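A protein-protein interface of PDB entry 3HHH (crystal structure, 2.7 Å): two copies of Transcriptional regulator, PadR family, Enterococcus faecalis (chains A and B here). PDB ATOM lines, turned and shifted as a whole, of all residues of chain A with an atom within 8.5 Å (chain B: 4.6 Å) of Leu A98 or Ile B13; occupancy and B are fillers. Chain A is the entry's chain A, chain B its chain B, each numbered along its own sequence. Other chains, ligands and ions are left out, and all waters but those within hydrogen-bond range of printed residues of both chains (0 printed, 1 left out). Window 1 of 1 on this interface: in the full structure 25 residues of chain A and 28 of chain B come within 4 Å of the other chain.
The backbone carbonyl oxygen (O) of Glu A8 sits close to the backbone carbonyl oxygen (O) of Lys B11 (2.9 Å).
NE1 of Trp B95 lies within hydrogen-bond range of OD1 of Asn A103, 3.1 Å away.
The side-chain carboxylate (OE2) of Glu A8 is in salt-bridge range of the side-chain amino group (NZ) of Lys A11 (2.5 Å).
The side-chain amide nitrogen of Asn A103 lies close to the backbone carbonyl oxygen of Ser A99 (3.3 Å).
The backbone NH (N) of Gly B12 is in hydrogen-bond range of the side-chain carboxylate (OE1) of Glu B15, at 3.1 Å.
O of Thr A96 is in hydrogen-bond range of OG of Ser A99, at 3.5 Å.
The side-chain hydroxyl (OG) of Ser A99 is in hydrogen-bond range of the backbone carbonyl oxygen (O) of Trp A95, at 3.3 Å.
Glu B15 touches Lys A5 (CB to NZ, 3.5 Å).
Leu A9 touches Gly B12.
N of Ile B13 touches CD1 of Leu A9, at 3.9 Å.
Leu B9 touches Lys A11.
Lys B11 touches Lys A11 (CD to CD, 3.7 Å).
Trp A95 touches Trp B95 (CH2 to CH2, 3.8 Å).
Leu B10 touches Leu A98 (CD2 to CD1, 3.9 Å).
Leu A98 touches Ile B13.
Val A102 touches Ile B13 (CG2 to CG2, 3.9 Å).
Trp B95 touches Val A102 (CE2 to CG1, 3.4 Å).
Printed residues of chain B within 4 Å of Leu A98: Leu B9 (3.7 Å), Leu B10 (3.9 Å), Ile B13 (3.4 Å) and Phe B41 (3.6 Å).
Ile B13 touches just these residues of chain A: Leu A9, Leu A98 and Val A102.
Printed residues of chain B within 4 Å of Glu A8: Lys B11 (2.9 Å).
Printed residues of chain B within 4 Å of Leu A9: Lys B11 (3.9 Å), Gly B12 (3.8 Å) and Ile B13 (3.9 Å).
Leu B14 touches none of the printed residues of chain A.
Lys A100 touches none of the printed residues of chain B.
The nearest residue of chain A that does not touch Ile B13 is Ile A13 (5.3 Å).
Of the 22 printed residues of chain A, 11 touch a printed residue of chain B.
Printed residues of chain A that touch a printed residue of chain B: Lys A5, Glu A8, Leu A9, Lys A11, Ile A13, Trp A95, Leu A98, Ser A99, Gln A101, Val A102 and Asn A103.
Hydrophobic or aromatic side chains of chain A that line the printed part of chain B: Leu A9, Ile A13, Trp A95, Leu A98 and Val A102.
Hydrophobic or aromatic side chains of chain B that line the printed part of chain A: Leu B9, Leu B10, Ile B13, Phe B41 and Trp B95.
Among the printed residues, no Asp or Glu carboxylate lies within 4 Å of a Lys or Arg side-chain nitrogen of the other chain.
Leu A9 touches Lys B11, and with the chains exchanged Lys A11 touches Leu B9.
Leu A9 touches Gly B12, but with the chains exchanged Gly A12 does not touch Leu B9 (4.2 Å).
Leu A9 touches Ile B13, and with the chains exchanged Ile A13 touches Leu B9.
Trp B95 touches its own counterpart, Trp A95.
Of the 19 pairs that touch across the chains among the printed residues, 6 have their exchanged pair printed and touching as well.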
ATOM      1  N   LYS A   5      24.567  19.508  26.309  1.00  0.00           N
ATOM      2  CA  LYS A   5      23.592  20.552  26.750  1.00  0.00           C
ATOM      3  C   LYS A   5      22.138  20.086  26.560  1.00  0.00           C
ATOM      4  O   LYS A   5      21.216  20.715  27.078  1.00  0.00           O
ATOM      5  CB  LYS A   5      23.837  21.867  25.992  1.00  0.00           C
ATOM      6  CG  LYS A   5      23.514  23.136  26.781  1.00  0.00           C
ATOM      7  CD  LYS A   5      23.822  24.407  25.967  1.00  0.00           C
ATOM      8  CE  LYS A   5      25.305  24.781  26.008  1.00  0.00           C
ATOM      9  NZ  LYS A   5      25.699  25.393  27.305  1.00  0.00           N
ATOM     10  N   GLU A   8      20.523  19.085  29.864  1.00  0.00           N
ATOM     11  CA  GLU A   8      20.075  20.298  30.550  1.00  0.00           C
ATOM     12  C   GLU A   8      18.858  20.945  29.877  1.00  0.00           C
ATOM     13  O   GLU A   8      18.067  21.619  30.535  1.00  0.00           O
ATOM     14  CB  GLU A   8      21.220  21.312  30.627  1.00  0.00           C
ATOM     15  CG  GLU A   8      22.345  20.899  31.563  1.00  0.00           C
ATOM     16  CD  GLU A   8      22.163  21.420  32.980  1.00  0.00           C
ATOM     17  OE1 GLU A   8      22.066  22.655  33.155  1.00  0.00           O
ATOM     18  OE2 GLU A   8      22.138  20.601  33.923  1.00  0.00           O
ATOM     19  N   LEU A   9      18.712  20.740  28.571  1.00  0.00           N
ATOM     20  CA  LEU A   9      17.595  21.316  27.813  1.00  0.00           C
ATOM     21  C   LEU A   9      16.258  20.654  28.174  1.00  0.00           C
ATOM     22  O   LEU A   9      15.217  21.312  28.209  1.00  0.00           O
ATOM     23  CB  LEU A   9      17.851  21.183  26.307  1.00  0.00           C
ATOM     24  CG  LEU A   9      17.292  22.310  25.443  1.00  0.00           C
ATOM     25  CD1 LEU A   9      18.084  23.593  25.667  1.00  0.00           C
ATOM     26  CD2 LEU A   9      17.318  21.909  23.976  1.00  0.00           C
ATOM     27  N   LEU A  10      16.307  19.351  28.437  1.00  0.00           N
ATOM     28  CA  LEU A  10      15.124  18.579  28.789  1.00  0.00           C
ATOM     29  C   LEU A  10      14.720  18.784  30.249  1.00  0.00           C
ATOM     30  O   LEU A  10      13.584  18.489  30.627  1.00  0.00           O
ATOM     31  CB  LEU A  10      15.372  17.093  28.526  1.00  0.00           C
ATOM     32  CG  LEU A  10      15.597  16.707  27.063  1.00  0.00           C
ATOM     33  CD1 LEU A  10      16.184  15.293  26.943  1.00  0.00           C
ATOM     34  CD2 LEU A  10      14.294  16.830  26.282  1.00  0.00           C
ATOM     35  N   LYS A  11      15.642  19.279  31.071  1.00  0.00           N
ATOM     36  CA  LYS A  11      15.345  19.525  32.481  1.00  0.00           C
ATOM     37  C   LYS A  11      14.175  20.501  32.634  1.00  0.00           C
ATOM     38  O   LYS A  11      14.147  21.557  32.000  1.00  0.00           O
ATOM     39  CB  LYS A  11      16.583  20.044  33.218  1.00  0.00           C
ATOM     40  CG  LYS A  11      17.691  19.003  33.365  1.00  0.00           C
ATOM     41  CD  LYS A  11      18.833  19.522  34.230  1.00  0.00           C
ATOM     42  CE  LYS A  11      19.881  18.445  34.498  1.00  0.00           C
ATOM     43  NZ  LYS A  11      20.963  18.928  35.415  1.00  0.00           N
ATOM     44  N   GLY A  12      13.204  20.127  33.463  1.00  0.00           N
ATOM     45  CA  GLY A  12      11.975  20.897  33.624  1.00  0.00           C
ATOM     46  C   GLY A  12      10.948  20.421  32.622  1.00  0.00           C
ATOM     47  O   GLY A  12       9.874  19.946  32.995  1.00  0.00           O
ATOM     48  N   ILE A  13      11.296  20.530  31.343  1.00  0.00           N
ATOM     49  CA  ILE A  13      10.423  20.111  30.250  1.00  0.00           C
ATOM     50  C   ILE A  13       9.980  18.661  30.412  1.00  0.00           C
ATOM     51  O   ILE A  13       8.788  18.366  30.409  1.00  0.00           O
ATOM     52  CB  ILE A  13      11.125  20.258  28.876  1.00  0.00           C
ATOM     53  CG1 ILE A  13      11.401  21.735  28.563  1.00  0.00           C
ATOM     54  CG2 ILE A  13      10.271  19.646  27.777  1.00  0.00           C
ATOM     55  CD1 ILE A  13      12.147  21.956  27.258  1.00  0.00           C
ATOM     56  N   PHE A  91       2.349  24.028  33.787  1.00  0.00           N
ATOM     57  CA  PHE A  91       3.485  23.805  32.897  1.00  0.00           C
ATOM     58  C   PHE A  91       3.229  24.345  31.489  1.00  0.00           C
ATOM     59  O   PHE A  91       4.101  24.993  30.906  1.00  0.00           O
ATOM     60  CB  PHE A  91       3.852  22.314  32.845  1.00  0.00           C
ATOM     61  CG  PHE A  91       4.701  21.942  31.666  1.00  0.00           C
ATOM     62  CD1 PHE A  91       6.023  22.351  31.591  1.00  0.00           C
ATOM     63  CD2 PHE A  91       4.174  21.198  30.621  1.00  0.00           C
ATOM     64  CE1 PHE A  91       6.807  22.018  30.495  1.00  0.00           C
ATOM     65  CE2 PHE A  91       4.951  20.860  29.526  1.00  0.00           C
ATOM     66  CZ  PHE A  91       6.267  21.271  29.460  1.00  0.00           C
ATOM     67  N   TRP A  92       2.042  24.084  30.944  1.00  0.00           N
ATOM     68  CA  TRP A  92       1.702  24.567  29.602  1.00  0.00           C
ATOM     69  C   TRP A  92       1.676  26.094  29.540  1.00  0.00           C
ATOM     70  O   TRP A  92       2.162  26.690  28.579  1.00  0.00           O
ATOM     71  CB  TRP A  92       0.356  24.002  29.137  1.00  0.00           C
ATOM     72  CG  TRP A  92       0.373  22.529  28.872  1.00  0.00           C
ATOM     73  CD1 TRP A  92      -0.461  21.589  29.411  1.00  0.00           C
ATOM     74  CD2 TRP A  92       1.266  21.823  28.001  1.00  0.00           C
ATOM     75  NE1 TRP A  92      -0.141  20.340  28.930  1.00  0.00           N
ATOM     76  CE2 TRP A  92       0.916  20.456  28.063  1.00  0.00           C
ATOM     77  CE3 TRP A  92       2.330  22.212  27.176  1.00  0.00           C
ATOM     78  CZ2 TRP A  92       1.592  19.475  27.332  1.00  0.00           C
ATOM     79  CZ3 TRP A  92       3.001  21.240  26.452  1.00  0.00           C
ATOM     80  CH2 TRP A  92       2.628  19.886  26.534  1.00  0.00           C
ATOM     81  N   GLN A  93       1.109  26.715  30.571  1.00  0.00           N
ATOM     82  CA  GLN A  93       1.078  28.171  30.700  1.00  0.00           C
ATOM     83  C   GLN A  93       2.486  28.771  30.633  1.00  0.00           C
ATOM     84  O   GLN A  93       2.739  29.694  29.853  1.00  0.00           O
ATOM     85  CB  GLN A  93       0.399  28.559  32.019  1.00  0.00           C
ATOM     86  CG  GLN A  93       0.440  30.044  32.355  1.00  0.00           C
ATOM     87  CD  GLN A  93      -0.290  30.376  33.648  1.00  0.00           C
ATOM     88  OE1 GLN A  93      -1.111  31.299  33.691  1.00  0.00           O
ATOM     89  NE2 GLN A  93       0.007  29.626  34.711  1.00  0.00           N
ATOM     90  N   ARG A  94       3.388  28.239  31.449  1.00  0.00           N
ATOM     91  CA  ARG A  94       4.768  28.729  31.511  1.00  0.00           C
ATOM     92  C   ARG A  94       5.576  28.394  30.254  1.00  0.00           C
ATOM     93  O   ARG A  94       6.376  29.212  29.792  1.00  0.00           O
ATOM     94  CB  ARG A  94       5.481  28.173  32.746  1.00  0.00           C
ATOM     95  CG  ARG A  94       5.012  28.802  34.045  1.00  0.00           C
ATOM     96  CD  ARG A  94       5.837  28.316  35.212  1.00  0.00           C
ATOM     97  NE  ARG A  94       5.433  26.984  35.659  1.00  0.00           N
ATOM     98  CZ  ARG A  94       6.231  26.114  36.275  1.00  0.00           C
ATOM     99  NH1 ARG A  94       7.506  26.407  36.514  1.00  0.00           N
ATOM    100  NH2 ARG A  94       5.753  24.929  36.640  1.00  0.00           N
ATOM    101  N   TRP A  95       5.371  27.195  29.715  1.00  0.00           N
ATOM    102  CA  TRP A  95       6.029  26.788  28.479  1.00  0.00           C
ATOM    103  C   TRP A  95       5.641  27.706  27.333  1.00  0.00           C
ATOM    104  O   TRP A  95       6.504  28.161  26.586  1.00  0.00           O
ATOM    105  CB  TRP A  95       5.680  25.347  28.100  1.00  0.00           C
ATOM    106  CG  TRP A  95       6.024  25.052  26.673  1.00  0.00           C
ATOM    107  CD1 TRP A  95       5.164  25.024  25.610  1.00  0.00           C
ATOM    108  CD2 TRP A  95       7.327  24.789  26.142  1.00  0.00           C
ATOM    109  NE1 TRP A  95       5.851  24.743  24.456  1.00  0.00           N
ATOM    110  CE2 TRP A  95       7.181  24.595  24.754  1.00  0.00           C
ATOM    111  CE3 TRP A  95       8.605  24.689  26.708  1.00  0.00           C
ATOM    112  CZ2 TRP A  95       8.262  24.309  23.920  1.00  0.00           C
ATOM    113  CZ3 TRP A  95       9.678  24.399  25.880  1.00  0.00           C
ATOM    114  CH2 TRP A  95       9.500  24.216  24.500  1.00  0.00           C
ATOM    115  N   THR A  96       4.342  27.956  27.186  1.00  0.00           N
ATOM    116  CA  THR A  96       3.838  28.858  26.151  1.00  0.00           C
ATOM    117  C   THR A  96       4.556  30.204  26.217  1.00  0.00           C
ATOM    118  O   THR A  96       5.010  30.734  25.200  1.00  0.00           O
ATOM    119  CB  THR A  96       2.323  29.093  26.307  1.00  0.00           C
ATOM    120  OG1 THR A  96       1.637  27.840  26.211  1.00  0.00           O
ATOM    121  CG2 THR A  96       1.804  30.036  25.229  1.00  0.00           C
ATOM    122  N   LEU A  97       4.662  30.726  27.435  1.00  0.00           N
ATOM    123  CA  LEU A  97       5.331  31.988  27.704  1.00  0.00           C
ATOM    124  C   LEU A  97       6.825  31.911  27.378  1.00  0.00           C
ATOM    125  O   LEU A  97       7.363  32.793  26.712  1.00  0.00           O
ATOM    126  CB  LEU A  97       5.130  32.355  29.177  1.00  0.00           C
ATOM    127  CG  LEU A  97       5.337  33.807  29.601  1.00  0.00           C
ATOM    128  CD1 LEU A  97       4.579  34.773  28.694  1.00  0.00           C
ATOM    129  CD2 LEU A  97       4.888  33.965  31.042  1.00  0.00           C
ATOM    130  N   LEU A  98       7.481  30.845  27.828  1.00  0.00           N
ATOM    131  CA  LEU A  98       8.925  30.687  27.642  1.00  0.00           C
ATOM    132  C   LEU A  98       9.338  30.626  26.169  1.00  0.00           C
ATOM    133  O   LEU A  98      10.320  31.257  25.775  1.00  0.00           O
ATOM    134  CB  LEU A  98       9.427  29.431  28.361  1.00  0.00           C
ATOM    135  CG  LEU A  98      10.951  29.259  28.405  1.00  0.00           C
ATOM    136  CD1 LEU A  98      11.568  30.194  29.430  1.00  0.00           C
ATOM    137  CD2 LEU A  98      11.331  27.815  28.701  1.00  0.00           C
ATOM    138  N   SER A  99       8.608  29.855  25.365  1.00  0.00           N
ATOM    139  CA  SER A  99       8.961  29.677  23.953  1.00  0.00           C
ATOM    140  C   SER A  99       8.555  30.887  23.111  1.00  0.00           C
ATOM    141  O   SER A  99       9.178  31.168  22.091  1.00  0.00           O
ATOM    142  CB  SER A  99       8.336  28.403  23.386  1.00  0.00           C
ATOM    143  OG  SER A  99       6.934  28.521  23.324  1.00  0.00           O
ATOM    144  N   LYS A 100       7.510  31.595  23.535  1.00  0.00           N
ATOM    145  CA  LYS A 100       7.156  32.886  22.936  1.00  0.00           C
ATOM    146  C   LYS A 100       8.341  33.847  23.077  1.00  0.00           C
ATOM    147  O   LYS A 100       8.748  34.493  22.109  1.00  0.00           O
ATOM    148  CB  LYS A 100       5.913  33.467  23.620  1.00  0.00           C
ATOM    149  CG  LYS A 100       5.356  34.742  22.998  1.00  0.00           C
ATOM    150  CD  LYS A 100       4.243  35.338  23.874  1.00  0.00           C
ATOM    151  CE  LYS A 100       3.414  36.381  23.127  1.00  0.00           C
ATOM    152  NZ  LYS A 100       4.257  37.449  22.523  1.00  0.00           N
ATOM    153  N   GLN A 101       8.899  33.909  24.284  1.00  0.00           N
ATOM    154  CA  GLN A 101      10.037  34.776  24.589  1.00  0.00           C
ATOM    155  C   GLN A 101      11.340  34.316  23.927  1.00  0.00           C
ATOM    156  O   GLN A 101      12.123  35.145  23.469  1.00  0.00           O
ATOM    157  CB  GLN A 101      10.227  34.873  26.102  1.00  0.00           C
ATOM    158  CG  GLN A 101       9.075  35.578  26.811  1.00  0.00           C
ATOM    159  CD  GLN A 101       9.050  35.332  28.307  1.00  0.00           C
ATOM    160  OE1 GLN A 101       9.792  34.495  28.827  1.00  0.00           O
ATOM    161  NE2 GLN A 101       8.188  36.061  29.010  1.00  0.00           N
ATOM    162  N   VAL A 102      11.570  33.005  23.874  1.00  0.00           N
ATOM    163  CA  VAL A 102      12.777  32.458  23.241  1.00  0.00           C
ATOM    164  C   VAL A 102      12.746  32.624  21.713  1.00  0.00           C
ATOM    165  O   VAL A 102      13.749  33.011  21.109  1.00  0.00           O
ATOM    166  CB  VAL A 102      12.993  30.973  23.600  1.00  0.00           C
ATOM    167  CG1 VAL A 102      14.181  30.398  22.843  1.00  0.00           C
ATOM    168  CG2 VAL A 102      13.203  30.819  25.089  1.00  0.00           C
ATOM    169  N   ASN A 103      11.599  32.332  21.099  1.00  0.00           N
ATOM    170  CA  ASN A 103      11.415  32.563  19.661  1.00  0.00           C
ATOM    171  C   ASN A 103      11.573  34.036  19.288  1.00  0.00           C
ATOM    172  O   ASN A 103      12.128  34.355  18.237  1.00  0.00           O
ATOM    173  CB  ASN A 103      10.040  32.070  19.184  1.00  0.00           C
ATOM    174  CG  ASN A 103       9.953  30.556  19.075  1.00  0.00           C
ATOM    175  OD1 ASN A 103      10.963  29.859  18.985  1.00  0.00           O
ATOM    176  ND2 ASN A 103       8.732  30.040  19.068  1.00  0.00           N
ATOM    177  N   LYS A 104      11.087  34.930  20.147  1.00  0.00           N
ATOM    178  CA  LYS A 104      11.188  36.369  19.891  1.00  0.00           C
ATOM    179  C   LYS A 104      12.645  36.838  19.842  1.00  0.00           C
ATOM    180  O   LYS A 104      12.960  37.815  19.164  1.00  0.00           O
ATOM    181  CB  LYS A 104      10.418  37.170  20.943  1.00  0.00           C
ATOM    182  CG  LYS A 104      10.243  38.649  20.597  1.00  0.00           C
ATOM    183  CD  LYS A 104       9.793  39.463  21.802  1.00  0.00           C
ATOM    184  CE  LYS A 104      10.174  40.930  21.660  1.00  0.00           C
ATOM    185  NZ  LYS A 104       9.900  41.690  22.918  1.00  0.00           N
ATOM    186  N   MET A 105      13.529  36.143  20.554  1.00  0.00           N
ATOM    187  CA  MET A 105      14.945  36.498  20.561  1.00  0.00           C
ATOM    188  C   MET A 105      15.724  35.932  19.370  1.00  0.00           C
ATOM    189  O   MET A 105      16.729  36.515  18.966  1.00  0.00           O
ATOM    190  CB  MET A 105      15.584  36.097  21.889  1.00  0.00           C
ATOM    191  CG  MET A 105      15.096  36.958  23.042  1.00  0.00           C
ATOM    192  SD  MET A 105      16.291  37.002  24.578  1.00  0.00           S
ATOM    193  CE  MET A 105      18.004  37.254  23.668  1.00  0.00           C
ATOM    194  N   LEU B   9      13.574  24.753  34.084  1.00  0.00           N
ATOM    195  CA  LEU B   9      13.076  25.050  32.744  1.00  0.00           C
ATOM    196  C   LEU B   9      14.048  25.965  31.990  1.00  0.00           C
ATOM    197  O   LEU B   9      14.173  25.867  30.773  1.00  0.00           O
ATOM    198  CB  LEU B   9      11.682  25.687  32.844  1.00  0.00           C
ATOM    199  CG  LEU B   9      10.719  25.649  31.656  1.00  0.00           C
ATOM    200  CD1 LEU B   9      10.677  24.287  30.977  1.00  0.00           C
ATOM    201  CD2 LEU B   9       9.330  26.048  32.137  1.00  0.00           C
ATOM    202  N   LEU B  10      14.744  26.833  32.724  1.00  0.00           N
ATOM    203  CA  LEU B  10      15.703  27.772  32.136  1.00  0.00           C
ATOM    204  C   LEU B  10      17.092  27.165  31.890  1.00  0.00           C
ATOM    205  O   LEU B  10      17.914  27.770  31.192  1.00  0.00           O
ATOM    206  CB  LEU B  10      15.833  29.018  33.022  1.00  0.00           C
ATOM    207  CG  LEU B  10      14.682  30.026  32.903  1.00  0.00           C
ATOM    208  CD1 LEU B  10      14.629  30.967  34.109  1.00  0.00           C
ATOM    209  CD2 LEU B  10      14.799  30.818  31.605  1.00  0.00           C
ATOM    210  N   LYS B  11      17.361  25.988  32.460  1.00  0.00           N
ATOM    211  CA  LYS B  11      18.656  25.327  32.268  1.00  0.00           C
ATOM    212  C   LYS B  11      18.848  24.953  30.804  1.00  0.00           C
ATOM    213  O   LYS B  11      17.917  24.475  30.159  1.00  0.00           O
ATOM    214  CB  LYS B  11      18.785  24.072  33.142  1.00  0.00           C
ATOM    215  CG  LYS B  11      19.154  24.341  34.592  1.00  0.00           C
ATOM    216  CD  LYS B  11      19.250  23.036  35.381  1.00  0.00           C
ATOM    217  CE  LYS B  11      19.723  23.267  36.815  1.00  0.00           C
ATOM    218  NZ  LYS B  11      20.018  21.984  37.530  1.00  0.00           N
ATOM    219  N   GLY B  12      20.050  25.182  30.279  1.00  0.00           N
ATOM    220  CA  GLY B  12      20.348  24.897  28.877  1.00  0.00           C
ATOM    221  C   GLY B  12      19.905  26.020  27.958  1.00  0.00           C
ATOM    222  O   GLY B  12      20.649  26.425  27.062  1.00  0.00           O
ATOM    223  N   ILE B  13      18.693  26.522  28.180  1.00  0.00           N
ATOM    224  CA  ILE B  13      18.143  27.622  27.403  1.00  0.00           C
ATOM    225  C   ILE B  13      18.885  28.918  27.693  1.00  0.00           C
ATOM    226  O   ILE B  13      19.257  29.642  26.775  1.00  0.00           O
ATOM    227  CB  ILE B  13      16.646  27.853  27.717  1.00  0.00           C
ATOM    228  CG1 ILE B  13      15.829  26.580  27.453  1.00  0.00           C
ATOM    229  CG2 ILE B  13      16.101  29.027  26.895  1.00  0.00           C
ATOM    230  CD1 ILE B  13      14.340  26.759  27.647  1.00  0.00           C
ATOM    231  N   LEU B  14      19.098  29.207  28.971  1.00  0.00           N
ATOM    232  CA  LEU B  14      19.677  30.486  29.377  1.00  0.00           C
ATOM    233  C   LEU B  14      21.075  30.683  28.806  1.00  0.00           C
ATOM    234  O   LEU B  14      21.414  31.781  28.359  1.00  0.00           O
ATOM    235  CB  LEU B  14      19.699  30.610  30.900  1.00  0.00           C
ATOM    236  CG  LEU B  14      19.984  32.014  31.441  1.00  0.00           C
ATOM    237  CD1 LEU B  14      19.050  33.049  30.823  1.00  0.00           C
ATOM    238  CD2 LEU B  14      19.875  32.023  32.969  1.00  0.00           C
ATOM    239  N   GLU B  15      21.877  29.619  28.817  1.00  0.00           N
ATOM    240  CA  GLU B  15      23.184  29.626  28.153  1.00  0.00           C
ATOM    241  C   GLU B  15      23.028  30.051  26.696  1.00  0.00           C
ATOM    242  O   GLU B  15      23.785  30.881  26.196  1.00  0.00           O
ATOM    243  CB  GLU B  15      23.844  28.242  28.205  1.00  0.00           C
ATOM    244  CG  GLU B  15      24.488  27.872  29.551  1.00  0.00           C
ATOM    245  CD  GLU B  15      23.518  27.269  30.576  1.00  0.00           C
ATOM    246  OE1 GLU B  15      22.280  27.336  30.378  1.00  0.00           O
ATOM    247  OE2 GLU B  15      24.012  26.726  31.592  1.00  0.00           O
ATOM    248  N   GLY B  16      22.031  29.479  26.025  1.00  0.00           N
ATOM    249  CA  GLY B  16      21.762  29.785  24.625  1.00  0.00           C
ATOM    250  C   GLY B  16      21.366  31.229  24.401  1.00  0.00           C
ATOM    251  O   GLY B  16      21.830  31.861  23.458  1.00  0.00           O
ATOM    252  N   LEU B  17      20.501  31.745  25.267  1.00  0.00           N
ATOM    253  CA  LEU B  17      20.057  33.133  25.177  1.00  0.00           C
ATOM    254  C   LEU B  17      21.189  34.110  25.479  1.00  0.00           C
ATOM    255  O   LEU B  17      21.264  35.182  24.886  1.00  0.00           O
ATOM    256  CB  LEU B  17      18.897  33.387  26.144  1.00  0.00           C
ATOM    257  CG  LEU B  17      17.598  32.621  25.895  1.00  0.00           C
ATOM    258  CD1 LEU B  17      16.560  33.035  26.928  1.00  0.00           C
ATOM    259  CD2 LEU B  17      17.080  32.856  24.471  1.00  0.00           C
ATOM    260  N   PHE B  41      12.538  37.725  31.073  1.00  0.00           N
ATOM    261  CA  PHE B  41      12.921  36.718  32.051  1.00  0.00           C
ATOM    262  C   PHE B  41      13.242  37.475  33.337  1.00  0.00           C
ATOM    263  O   PHE B  41      14.403  37.716  33.670  1.00  0.00           O
ATOM    264  CB  PHE B  41      14.112  35.900  31.545  1.00  0.00           C
ATOM    265  CG  PHE B  41      13.879  35.271  30.198  1.00  0.00           C
ATOM    266  CD1 PHE B  41      14.259  35.928  29.034  1.00  0.00           C
ATOM    267  CD2 PHE B  41      13.260  34.030  30.092  1.00  0.00           C
ATOM    268  CE1 PHE B  41      14.034  35.358  27.785  1.00  0.00           C
ATOM    269  CE2 PHE B  41      13.033  33.449  28.847  1.00  0.00           C
ATOM    270  CZ  PHE B  41      13.420  34.115  27.692  1.00  0.00           C
ATOM    271  N   PHE B  91      22.516  25.691  19.140  1.00  0.00           N
ATOM    272  CA  PHE B  91      21.450  25.873  20.126  1.00  0.00           C
ATOM    273  C   PHE B  91      20.103  26.116  19.456  1.00  0.00           C
ATOM    274  O   PHE B  91      19.109  25.483  19.814  1.00  0.00           O
ATOM    275  CB  PHE B  91      21.769  27.018  21.100  1.00  0.00           C
ATOM    276  CG  PHE B  91      20.556  27.564  21.810  1.00  0.00           C
ATOM    277  CD1 PHE B  91      19.829  26.769  22.680  1.00  0.00           C
ATOM    278  CD2 PHE B  91      20.134  28.876  21.593  1.00  0.00           C
ATOM    279  CE1 PHE B  91      18.704  27.269  23.329  1.00  0.00           C
ATOM    280  CE2 PHE B  91      19.011  29.383  22.238  1.00  0.00           C
ATOM    281  CZ  PHE B  91      18.299  28.580  23.108  1.00  0.00           C
ATOM    282  N   TRP B  95      16.946  23.800  19.696  1.00  0.00           N
ATOM    283  CA  TRP B  95      15.759  24.432  20.252  1.00  0.00           C
ATOM    284  C   TRP B  95      14.582  24.333  19.291  1.00  0.00           C
ATOM    285  O   TRP B  95      13.478  23.980  19.697  1.00  0.00           O
ATOM    286  CB  TRP B  95      16.022  25.901  20.600  1.00  0.00           C
ATOM    287  CG  TRP B  95      14.761  26.690  20.759  1.00  0.00           C
ATOM    288  CD1 TRP B  95      14.205  27.527  19.843  1.00  0.00           C
ATOM    289  CD2 TRP B  95      13.884  26.689  21.887  1.00  0.00           C
ATOM    290  NE1 TRP B  95      13.042  28.062  20.332  1.00  0.00           N
ATOM    291  CE2 TRP B  95      12.820  27.563  21.587  1.00  0.00           C
ATOM    292  CE3 TRP B  95      13.896  26.039  23.124  1.00  0.00           C
ATOM    293  CZ2 TRP B  95      11.773  27.805  22.479  1.00  0.00           C
ATOM    294  CZ3 TRP B  95      12.857  26.282  24.015  1.00  0.00           C
ATOM    295  CH2 TRP B  95      11.811  27.157  23.685  1.00  0.00           C
